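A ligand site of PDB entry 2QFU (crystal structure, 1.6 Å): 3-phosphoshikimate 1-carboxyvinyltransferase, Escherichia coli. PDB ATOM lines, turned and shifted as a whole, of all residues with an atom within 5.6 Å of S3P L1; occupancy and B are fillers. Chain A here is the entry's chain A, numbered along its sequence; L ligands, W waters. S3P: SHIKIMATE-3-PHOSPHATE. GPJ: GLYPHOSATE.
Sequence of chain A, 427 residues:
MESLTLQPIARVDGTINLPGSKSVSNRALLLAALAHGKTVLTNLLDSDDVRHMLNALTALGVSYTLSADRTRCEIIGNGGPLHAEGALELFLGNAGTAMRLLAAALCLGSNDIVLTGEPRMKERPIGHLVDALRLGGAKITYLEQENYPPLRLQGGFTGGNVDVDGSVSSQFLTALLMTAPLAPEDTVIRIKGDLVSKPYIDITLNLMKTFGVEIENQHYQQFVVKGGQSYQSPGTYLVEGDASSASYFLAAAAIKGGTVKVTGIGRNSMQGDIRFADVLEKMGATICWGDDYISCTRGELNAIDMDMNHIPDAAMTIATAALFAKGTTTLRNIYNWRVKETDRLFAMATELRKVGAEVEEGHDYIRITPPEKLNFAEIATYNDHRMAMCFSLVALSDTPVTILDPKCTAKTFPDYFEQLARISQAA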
ATOM      1  N   LYS A  22     -10.741 -36.799  -6.826  1.00  0.00           N
ATOM      2  CA  LYS A  22     -10.637 -35.729  -7.821  1.00  0.00           C
ATOM      3  C   LYS A  22      -9.262 -35.049  -7.712  1.00  0.00           C
ATOM      4  O   LYS A  22      -8.602 -34.784  -8.715  1.00  0.00           O
ATOM      5  CB  LYS A  22     -11.746 -34.678  -7.570  1.00  0.00           C
ATOM      6  CG  LYS A  22     -11.628 -33.425  -8.454  1.00  0.00           C
ATOM      7  CD  LYS A  22     -11.345 -32.154  -7.644  1.00  0.00           C
ATOM      8  CE  LYS A  22     -12.612 -31.698  -6.920  1.00  0.00           C
ATOM      9  NZ  LYS A  22     -12.283 -30.653  -5.910  1.00  0.00           N
ATOM     10  N   SER A  23      -8.831 -34.799  -6.469  1.00  0.00           N
ATOM     11  CA  SER A  23      -7.547 -34.137  -6.244  1.00  0.00           C
ATOM     12  C   SER A  23      -6.371 -34.937  -6.791  1.00  0.00           C
ATOM     13  O   SER A  23      -5.477 -34.389  -7.457  1.00  0.00           O
ATOM     14  CB  SER A  23      -7.347 -33.908  -4.739  1.00  0.00           C
ATOM     15  OG  SER A  23      -8.265 -32.949  -4.264  1.00  0.00           O
ATOM     16  N   ARG A  27      -4.086 -34.153 -10.542  1.00  0.00           N
ATOM     17  CA  ARG A  27      -2.637 -33.991 -10.437  1.00  0.00           C
ATOM     18  C   ARG A  27      -1.962 -35.099 -11.243  1.00  0.00           C
ATOM     19  O   ARG A  27      -0.999 -34.849 -11.974  1.00  0.00           O
ATOM     20  CB  ARG A  27      -2.197 -34.142  -8.978  1.00  0.00           C
ATOM     21  CG  ARG A  27      -2.481 -32.917  -8.130  1.00  0.00           C
ATOM     22  CD  ARG A  27      -2.205 -33.284  -6.690  1.00  0.00           C
ATOM     23  NE  ARG A  27      -2.295 -32.192  -5.740  1.00  0.00           N
ATOM     24  CZ  ARG A  27      -3.435 -31.622  -5.338  1.00  0.00           C
ATOM     25  NH1 ARG A  27      -3.383 -30.640  -4.434  1.00  0.00           N
ATOM     26  NH2 ARG A  27      -4.607 -31.984  -5.863  1.00  0.00           N
ATOM     27  N   THR A  97      -8.992 -27.207  -9.714  1.00  0.00           N
ATOM     28  CA  THR A  97      -7.749 -27.967  -9.825  1.00  0.00           C
ATOM     29  C   THR A  97      -7.221 -27.911 -11.238  1.00  0.00           C
ATOM     30  O   THR A  97      -6.008 -27.911 -11.437  1.00  0.00           O
ATOM     31  CB  THR A  97      -7.907 -29.435  -9.355  1.00  0.00           C
ATOM     32  OG1 THR A  97      -8.992 -30.088 -10.040  1.00  0.00           O
ATOM     33  CG2 THR A  97      -8.172 -29.476  -7.863  1.00  0.00           C
ATOM     34  N   ARG A 100      -6.196 -23.740 -11.825  1.00  0.00           N
ATOM     35  CA  ARG A 100      -4.990 -23.286 -11.147  1.00  0.00           C
ATOM     36  C   ARG A 100      -3.752 -24.045 -11.609  1.00  0.00           C
ATOM     37  O   ARG A 100      -2.721 -23.430 -11.893  1.00  0.00           O
ATOM     38  CB  ARG A 100      -5.154 -23.417  -9.622  1.00  0.00           C
ATOM     39  CG  ARG A 100      -5.900 -22.249  -8.957  1.00  0.00           C
ATOM     40  CD  ARG A 100      -7.370 -22.197  -9.418  1.00  0.00           C
ATOM     41  NE  ARG A 100      -8.140 -21.170  -8.706  1.00  0.00           N
ATOM     42  CZ  ARG A 100      -8.801 -21.337  -7.559  1.00  0.00           C
ATOM     43  NH1 ARG A 100      -9.472 -20.310  -7.024  1.00  0.00           N
ATOM     44  NH2 ARG A 100      -8.812 -22.511  -6.935  1.00  0.00           N
ATOM     45  N   VAL A 168      -5.698 -17.701   0.730  1.00  0.00           N
ATOM     46  CA  VAL A 168      -6.999 -17.914   0.090  1.00  0.00           C
ATOM     47  C   VAL A 168      -7.121 -19.313  -0.513  1.00  0.00           C
ATOM     48  O   VAL A 168      -8.172 -19.961  -0.403  1.00  0.00           O
ATOM     49  CB  VAL A 168      -7.245 -16.835  -0.992  1.00  0.00           C
ATOM     50  CG1 VAL A 168      -8.494 -17.136  -1.788  1.00  0.00           C
ATOM     51  CG2 VAL A 168      -7.365 -15.466  -0.336  1.00  0.00           C
ATOM     52  N   SER A 169      -6.069 -19.786  -1.171  1.00  0.00           N
ATOM     53  CA  SER A 169      -6.100 -21.142  -1.735  1.00  0.00           C
ATOM     54  C   SER A 169      -4.745 -21.790  -1.692  1.00  0.00           C
ATOM     55  O   SER A 169      -3.729 -21.165  -2.009  1.00  0.00           O
ATOM     56  CB  SER A 169      -6.550 -21.144  -3.215  1.00  0.00           C
ATOM     57  OG  SER A 169      -6.618 -22.488  -3.715  1.00  0.00           O
ATOM     58  N   SER A 170      -4.719 -23.056  -1.308  1.00  0.00           N
ATOM     59  CA  SER A 170      -3.456 -23.790  -1.317  1.00  0.00           C
ATOM     60  C   SER A 170      -3.151 -24.189  -2.776  1.00  0.00           C
ATOM     61  O   SER A 170      -2.025 -24.573  -3.099  1.00  0.00           O
ATOM     62  CB  SER A 170      -3.577 -25.070  -0.479  1.00  0.00           C
ATOM     63  OG  SER A 170      -4.510 -25.998  -1.056  1.00  0.00           O
ATOM     64  N   GLN A 171      -4.146 -24.098  -3.653  1.00  0.00           N
ATOM     65  CA  GLN A 171      -3.907 -24.504  -5.026  1.00  0.00           C
ATOM     66  C   GLN A 171      -2.878 -23.669  -5.761  1.00  0.00           C
ATOM     67  O   GLN A 171      -2.245 -24.140  -6.715  1.00  0.00           O
ATOM     68  CB  GLN A 171      -5.209 -24.498  -5.822  1.00  0.00           C
ATOM     69  CG  GLN A 171      -6.162 -25.613  -5.388  1.00  0.00           C
ATOM     70  CD  GLN A 171      -7.413 -25.627  -6.229  1.00  0.00           C
ATOM     71  OE1 GLN A 171      -7.484 -24.982  -7.271  1.00  0.00           O
ATOM     72  NE2 GLN A 171      -8.412 -26.405  -5.799  1.00  0.00           N
ATOM     73  N   THR A 174       0.319 -25.237  -4.785  1.00  0.00           N
ATOM     74  CA  THR A 174       0.396 -26.531  -5.468  1.00  0.00           C
ATOM     75  C   THR A 174       0.800 -26.361  -6.929  1.00  0.00           C
ATOM     76  O   THR A 174       1.666 -27.086  -7.436  1.00  0.00           O
ATOM     77  CB  THR A 174      -0.973 -27.255  -5.404  1.00  0.00           C
ATOM     78  OG1 THR A 174      -1.026 -27.972  -4.177  1.00  0.00           O
ATOM     79  CG2 THR A 174      -1.169 -28.201  -6.588  1.00  0.00           C
ATOM     80  N   VAL A 196      -3.628 -21.864   4.013  1.00  0.00           N
ATOM     81  CA  VAL A 196      -4.846 -22.608   4.301  1.00  0.00           C
ATOM     82  C   VAL A 196      -4.829 -23.919   3.536  1.00  0.00           C
ATOM     83  O   VAL A 196      -4.017 -24.115   2.636  1.00  0.00           O
ATOM     84  CB  VAL A 196      -6.113 -21.811   3.887  1.00  0.00           C
ATOM     85  CG1 VAL A 196      -6.214 -20.535   4.707  1.00  0.00           C
ATOM     86  CG2 VAL A 196      -6.075 -21.499   2.381  1.00  0.00           C
ATOM     87  N   SER A 197      -5.711 -24.846   3.931  1.00  0.00           N
ATOM     88  CA  SER A 197      -5.832 -26.137   3.257  1.00  0.00           C
ATOM     89  C   SER A 197      -4.489 -26.833   3.108  1.00  0.00           C
ATOM     90  O   SER A 197      -4.214 -27.494   2.104  1.00  0.00           O
ATOM     91  CB  SER A 197      -6.454 -25.930   1.878  1.00  0.00           C
ATOM     92  OG  SER A 197      -7.811 -25.523   2.031  1.00  0.00           O
ATOM     93  N   TYR A 200      -3.505 -30.371   1.429  1.00  0.00           N
ATOM     94  CA  TYR A 200      -3.469 -30.598  -0.010  1.00  0.00           C
ATOM     95  C   TYR A 200      -2.063 -30.428  -0.560  1.00  0.00           C
ATOM     96  O   TYR A 200      -1.755 -30.965  -1.629  1.00  0.00           O
ATOM     97  CB  TYR A 200      -4.457 -29.680  -0.755  1.00  0.00           C
ATOM     98  CG  TYR A 200      -5.886 -30.100  -0.518  1.00  0.00           C
ATOM     99  CD1 TYR A 200      -6.633 -29.522   0.515  1.00  0.00           C
ATOM    100  CD2 TYR A 200      -6.484 -31.087  -1.301  1.00  0.00           C
ATOM    101  CE1 TYR A 200      -7.949 -29.941   0.767  1.00  0.00           C
ATOM    102  CE2 TYR A 200      -7.796 -31.499  -1.070  1.00  0.00           C
ATOM    103  CZ  TYR A 200      -8.515 -30.928  -0.048  1.00  0.00           C
ATOM    104  OH  TYR A 200      -9.818 -31.315   0.150  1.00  0.00           O
ATOM    105  N   ILE A 203      -0.539 -33.726  -0.599  1.00  0.00           N
ATOM    106  CA  ILE A 203      -0.967 -34.547  -1.723  1.00  0.00           C
ATOM    107  C   ILE A 203      -0.086 -34.197  -2.927  1.00  0.00           C
ATOM    108  O   ILE A 203       0.382 -35.079  -3.647  1.00  0.00           O
ATOM    109  CB  ILE A 203      -2.448 -34.254  -2.083  1.00  0.00           C
ATOM    110  CG1 ILE A 203      -3.350 -34.655  -0.913  1.00  0.00           C
ATOM    111  CG2 ILE A 203      -2.849 -35.045  -3.336  1.00  0.00           C
ATOM    112  CD1 ILE A 203      -4.841 -34.471  -1.223  1.00  0.00           C
ATOM    113  N   THR A 204       0.128 -32.912  -3.149  1.00  0.00           N
ATOM    114  CA  THR A 204       0.960 -32.457  -4.268  1.00  0.00           C
ATOM    115  C   THR A 204       2.371 -33.017  -4.211  1.00  0.00           C
ATOM    116  O   THR A 204       2.861 -33.553  -5.186  1.00  0.00           O
ATOM    117  CB  THR A 204       0.982 -30.936  -4.290  1.00  0.00           C
ATOM    118  OG1 THR A 204      -0.362 -30.491  -4.507  1.00  0.00           O
ATOM    119  CG2 THR A 204       1.875 -30.404  -5.440  1.00  0.00           C
ATOM    120  N   PRO A 312     -11.656 -28.426   4.705  1.00  0.00           N
ATOM    121  CA  PRO A 312     -12.725 -27.534   4.260  1.00  0.00           C
ATOM    122  C   PRO A 312     -13.887 -28.129   3.484  1.00  0.00           C
ATOM    123  O   PRO A 312     -15.042 -27.691   3.639  1.00  0.00           O
ATOM    124  CB  PRO A 312     -11.978 -26.449   3.472  1.00  0.00           C
ATOM    125  CG  PRO A 312     -10.823 -27.215   2.875  1.00  0.00           C
ATOM    126  CD  PRO A 312     -10.367 -28.071   4.072  1.00  0.00           C
ATOM    127  N   ASP A 313     -13.590 -29.118   2.653  1.00  0.00           N
ATOM    128  CA  ASP A 313     -14.633 -29.727   1.818  1.00  0.00           C
ATOM    129  C   ASP A 313     -15.488 -30.691   2.629  1.00  0.00           C
ATOM    130  O   ASP A 313     -16.704 -30.568   2.681  1.00  0.00           O
ATOM    131  CB  ASP A 313     -14.008 -30.456   0.627  1.00  0.00           C
ATOM    132  CG  ASP A 313     -13.303 -29.510  -0.334  1.00  0.00           C
ATOM    133  OD1 ASP A 313     -12.707 -30.033  -1.306  1.00  0.00           O
ATOM    134  OD2 ASP A 313     -13.345 -28.280  -0.139  1.00  0.00           O
ATOM    135  N   ASN A 336     -12.546 -19.647   3.138  1.00  0.00           N
ATOM    136  CA  ASN A 336     -12.563 -19.880   1.698  1.00  0.00           C
ATOM    137  C   ASN A 336     -13.733 -20.676   1.138  1.00  0.00           C
ATOM    138  O   ASN A 336     -13.834 -20.875  -0.079  1.00  0.00           O
ATOM    139  CB  ASN A 336     -11.178 -20.331   1.162  1.00  0.00           C
ATOM    140  CG  ASN A 336     -10.854 -21.786   1.411  1.00  0.00           C
ATOM    141  OD1 ASN A 336     -11.687 -22.583   1.870  1.00  0.00           O
ATOM    142  ND2 ASN A 336      -9.610 -22.149   1.077  1.00  0.00           N
ATOM    143  N   LYS A 340     -15.450 -20.731  -3.379  1.00  0.00           N
ATOM    144  CA  LYS A 340     -15.426 -22.006  -4.074  1.00  0.00           C
ATOM    145  C   LYS A 340     -16.596 -22.156  -5.052  1.00  0.00           C
ATOM    146  O   LYS A 340     -16.958 -21.157  -5.672  1.00  0.00           O
ATOM    147  CB  LYS A 340     -15.297 -23.140  -3.044  1.00  0.00           C
ATOM    148  CG  LYS A 340     -13.815 -23.229  -2.597  1.00  0.00           C
ATOM    149  CD  LYS A 340     -13.571 -24.128  -1.431  1.00  0.00           C
ATOM    150  CE  LYS A 340     -12.052 -24.209  -1.204  1.00  0.00           C
ATOM    151  NZ  LYS A 340     -11.757 -24.904   0.072  1.00  0.00           N
ATOM    152  N   GLU A 341     -17.194 -23.347  -5.195  1.00  0.00           N
ATOM    153  CA  GLU A 341     -18.263 -23.504  -6.200  1.00  0.00           C
ATOM    154  C   GLU A 341     -19.361 -22.484  -6.112  1.00  0.00           C
ATOM    155  O   GLU A 341     -19.957 -22.116  -7.133  1.00  0.00           O
ATOM    156  CB  GLU A 341     -18.833 -24.918  -6.156  1.00  0.00           C
ATOM    157  CG  GLU A 341     -17.887 -25.977  -6.799  1.00  0.00           C
ATOM    158  CD  GLU A 341     -16.736 -26.486  -5.899  1.00  0.00           C
ATOM    159  OE1 GLU A 341     -16.346 -25.795  -4.926  1.00  0.00           O
ATOM    160  OE2 GLU A 341     -16.210 -27.573  -6.203  1.00  0.00           O
ATOM    161  N   ARG A 344     -20.169 -20.783  -0.072  1.00  0.00           N
ATOM    162  CA  ARG A 344     -20.745 -21.838   0.751  1.00  0.00           C
ATOM    163  C   ARG A 344     -21.181 -21.440   2.139  1.00  0.00           C
ATOM    164  O   ARG A 344     -22.036 -22.090   2.728  1.00  0.00           O
ATOM    165  CB  ARG A 344     -19.776 -23.008   0.808  1.00  0.00           C
ATOM    166  CG  ARG A 344     -19.664 -23.689  -0.540  1.00  0.00           C
ATOM    167  CD  ARG A 344     -18.419 -24.595  -0.614  1.00  0.00           C
ATOM    168  NE  ARG A 344     -18.635 -25.652  -1.603  1.00  0.00           N
ATOM    169  CZ  ARG A 344     -17.756 -26.615  -1.886  1.00  0.00           C
ATOM    170  NH1 ARG A 344     -18.059 -27.528  -2.794  1.00  0.00           N
ATOM    171  NH2 ARG A 344     -16.577 -26.645  -1.252  1.00  0.00           N
ATOM    172  N   ARG A 386     -21.469 -30.342  -3.617  1.00  0.00           N
ATOM    173  CA  ARG A 386     -21.560 -30.621  -2.187  1.00  0.00           C
ATOM    174  C   ARG A 386     -22.809 -30.127  -1.495  1.00  0.00           C
ATOM    175  O   ARG A 386     -23.196 -30.655  -0.454  1.00  0.00           O
ATOM    176  CB  ARG A 386     -20.287 -30.139  -1.469  1.00  0.00           C
ATOM    177  CG  ARG A 386     -19.037 -30.881  -1.980  1.00  0.00           C
ATOM    178  CD  ARG A 386     -17.870 -30.920  -0.943  1.00  0.00           C
ATOM    179  NE  ARG A 386     -16.676 -31.306  -1.692  1.00  0.00           N
ATOM    180  CZ  ARG A 386     -16.425 -32.523  -2.168  1.00  0.00           C
ATOM    181  NH1 ARG A 386     -15.328 -32.696  -2.911  1.00  0.00           N
ATOM    182  NH2 ARG A 386     -17.177 -33.584  -1.844  1.00  0.00           N
HETATM  183  C1  S3P L   1      -7.904 -29.036  -3.610  1.00  0.00           C
HETATM  184  C2  S3P L   1      -7.673 -28.049  -2.640  1.00  0.00           C
HETATM  185  C3  S3P L   1      -8.816 -27.356  -1.940  1.00  0.00           C
HETATM  186  C4  S3P L   1     -10.156 -28.100  -2.090  1.00  0.00           C
HETATM  187  C5  S3P L   1     -10.375 -28.550  -3.539  1.00  0.00           C
HETATM  188  C6  S3P L   1      -9.228 -29.476  -3.949  1.00  0.00           C
HETATM  189  C7  S3P L   1      -6.725 -29.664  -4.298  1.00  0.00           C
HETATM  190  O1  S3P L   1      -8.865 -25.949  -2.337  1.00  0.00           O
HETATM  191  O2  S3P L   1     -11.217 -27.262  -1.587  1.00  0.00           O
HETATM  192  O3  S3P L   1     -11.621 -29.244  -3.672  1.00  0.00           O
HETATM  193  O4  S3P L   1      -5.635 -29.046  -4.273  1.00  0.00           O
HETATM  194  O5  S3P L   1      -6.876 -30.775  -4.799  1.00  0.00           O
HETATM  195  P1  S3P L   1      -8.290 -24.657  -1.450  1.00  0.00           P
HETATM  196  O6  S3P L   1      -6.830 -24.883  -1.301  1.00  0.00           O
HETATM  197  O7  S3P L   1      -9.032 -24.730  -0.136  1.00  0.00           O
HETATM  198  O8  S3P L   1      -8.599 -23.449  -2.262  1.00  0.00           O
HETATM  199  P1  GPJ L   2     -12.081 -26.630  -6.825  1.00  0.00           P
HETATM  200  O1  GPJ L   2     -11.611 -28.033  -6.879  1.00  0.00           O
HETATM  201  O2  GPJ L   2     -11.008 -25.618  -6.719  1.00  0.00           O
HETATM  202  O3  GPJ L   2     -13.018 -26.343  -7.983  1.00  0.00           O
HETATM  203  O4  GPJ L   2     -14.576 -29.944  -4.130  1.00  0.00           O
HETATM  204  O5  GPJ L   2     -15.586 -29.073  -2.370  1.00  0.00           O
HETATM  205  C1  GPJ L   2     -12.957 -26.413  -5.361  1.00  0.00           C
HETATM  206  C2  GPJ L   2     -14.346 -27.628  -3.668  1.00  0.00           C
HETATM  207  C3  GPJ L   2     -14.877 -28.980  -3.360  1.00  0.00           C
HETATM  208  N1  GPJ L   2     -13.562 -27.640  -4.905  1.00  0.00           N
HETATM  209  O   HOH W   1     -10.055 -21.294  -2.315  1.00  0.00           O
HETATM  210  O   HOH W   2      -3.614 -27.473  -3.306  1.00  0.00           O
HETATM  211  O   HOH W   3     -10.162 -23.779  -4.549  1.00  0.00           O
HETATM  212  O   HOH W   4     -11.115 -32.653  -4.132  1.00  0.00           O
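An oxygen (O6) of S3P L1 is in hydrogen-bond range of the backbone NH (N) of Ser 170 (2.8 Å).
The side-chain hydroxyl of Ser 170 lies within hydrogen-bond range of an oxygen (O6) of S3P L1 (2.6 Å).
OG of Ser 197 lies within hydrogen-bond range of O7 of S3P L1, at 2.6 Å.
An oxygen (O5) of S3P L1 lies within hydrogen-bond range of the side-chain hydroxyl (OG) of Ser 23, at 2.6 Å.
O8 of S3P L1 lies within hydrogen-bond range of OG of Ser 169, at 2.6 Å.
An oxygen (O3) of S3P L1 is in hydrogen-bond range of the side-chain carboxylate (OD1) of Asp 313, 2.7 Å away.
The side-chain amino group of Lys 22 sits at hydrogen-bond distance from an oxygen (O3) of S3P L1, 2.7 Å away.
O7 of S3P L1 lies within salt-bridge range of NZ of Lys 340 (2.7 Å).
O4 of S3P L1 lies within salt-bridge range of NH1 of Arg 27.
The side-chain amide nitrogen (ND2) of Asn 336 is in hydrogen-bond range of an oxygen (O7) of S3P L1, 2.9 Å away.
NZ of Lys 22 is in salt-bridge range of O1 of GPJ L2 (2.9 Å).
The side-chain amide nitrogen (NE2) of Gln 171 is in hydrogen-bond range of an oxygen (O2) of GPJ L2, at 2.9 Å.
The guanidinium group of Arg 100 lies within salt-bridge range of an oxygen (O2) of GPJ L2 (3.8 Å).
NE of Arg 386 is in salt-bridge range of O5 of GPJ L2, 2.6 Å away.
The guanidinium group (NH2) of Arg 344 lies within salt-bridge range of an oxygen (O5) of GPJ L2 (2.9 Å).
A nitrogen (N1) of GPJ L2 is in salt-bridge range of the side-chain carboxylate (OE2) of Glu 341, at 2.9 Å.
O3 of S3P L1 sits at hydrogen-bond distance from N1 of GPJ L2 (2.8 Å).
The backbone carbonyl oxygen (O) of Ser 23 is in hydrogen-bond range of the guanidinium group (NH2) of Arg 27 (3.0 Å).
OG of Ser 169 sits at hydrogen-bond distance from N of Gln 171 (3.0 Å).
The side-chain amino group of Lys 340 lies within salt-bridge range of the side-chain carboxylate of Asp 313 (3.7 Å).
The side-chain hydroxyl of Tyr 200 lies within hydrogen-bond range of the side-chain carboxylate of Asp 313, 3.5 Å away.
The side-chain amide oxygen (OD1) of Asn 336 is in hydrogen-bond range of the side-chain amino group (NZ) of Lys 340 (2.9 Å).
O of Tyr 200 sits at hydrogen-bond distance from NH1 of Arg 27 (3.3 Å).
The guanidinium group (NE) of Arg 27 lies within hydrogen-bond range of the side-chain hydroxyl (OG1) of Thr 204, 2.9 Å away.
OG1 of Thr 204 lies within hydrogen-bond range of O of Tyr 200, at 3.2 Å.
Residues that only touch S3P L1: Tyr 200, Gln 171, Thr 97 and Val 168.
Hydrophobic or aromatic side chains within 4 Å of S3P L1: Tyr 200.
Of the 22 residues printed, 13 come within 4 Å of S3P L1.
Along chain A the residues within 4 Å of S3P L1 span positions 22 to 340.
The nearest printed residue that does not touch S3P L1 is Pro 312 (4.3 Å).
Water W1 lies within hydrogen-bond range of O8 of S3P L1 and O of Val 168.
Water W2 lies within hydrogen-bond range of an oxygen (O4) of S3P L1, the side-chain hydroxyl (OG1) of Thr 174, the side-chain hydroxyl (OG) of Ser 170, the guanidinium group (NH1) of Arg 27 and the backbone NH (N) of Gln 171.
Water W3 lies within hydrogen-bond range of an oxygen (O8) of S3P L1 (2.8 Å), an oxygen (O2) of GPJ L2 (3.0 Å), the guanidinium group (NH2) of Arg 100 (3.0 Å) and the side-chain amide nitrogen (NE2) of Gln 171 (3.4 Å).
Water W4 lies within hydrogen-bond range of OG of Ser 23 (2.9 Å), NZ of Lys 22 (2.9 Å) and O3 of S3P L1 (3.5 Å).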
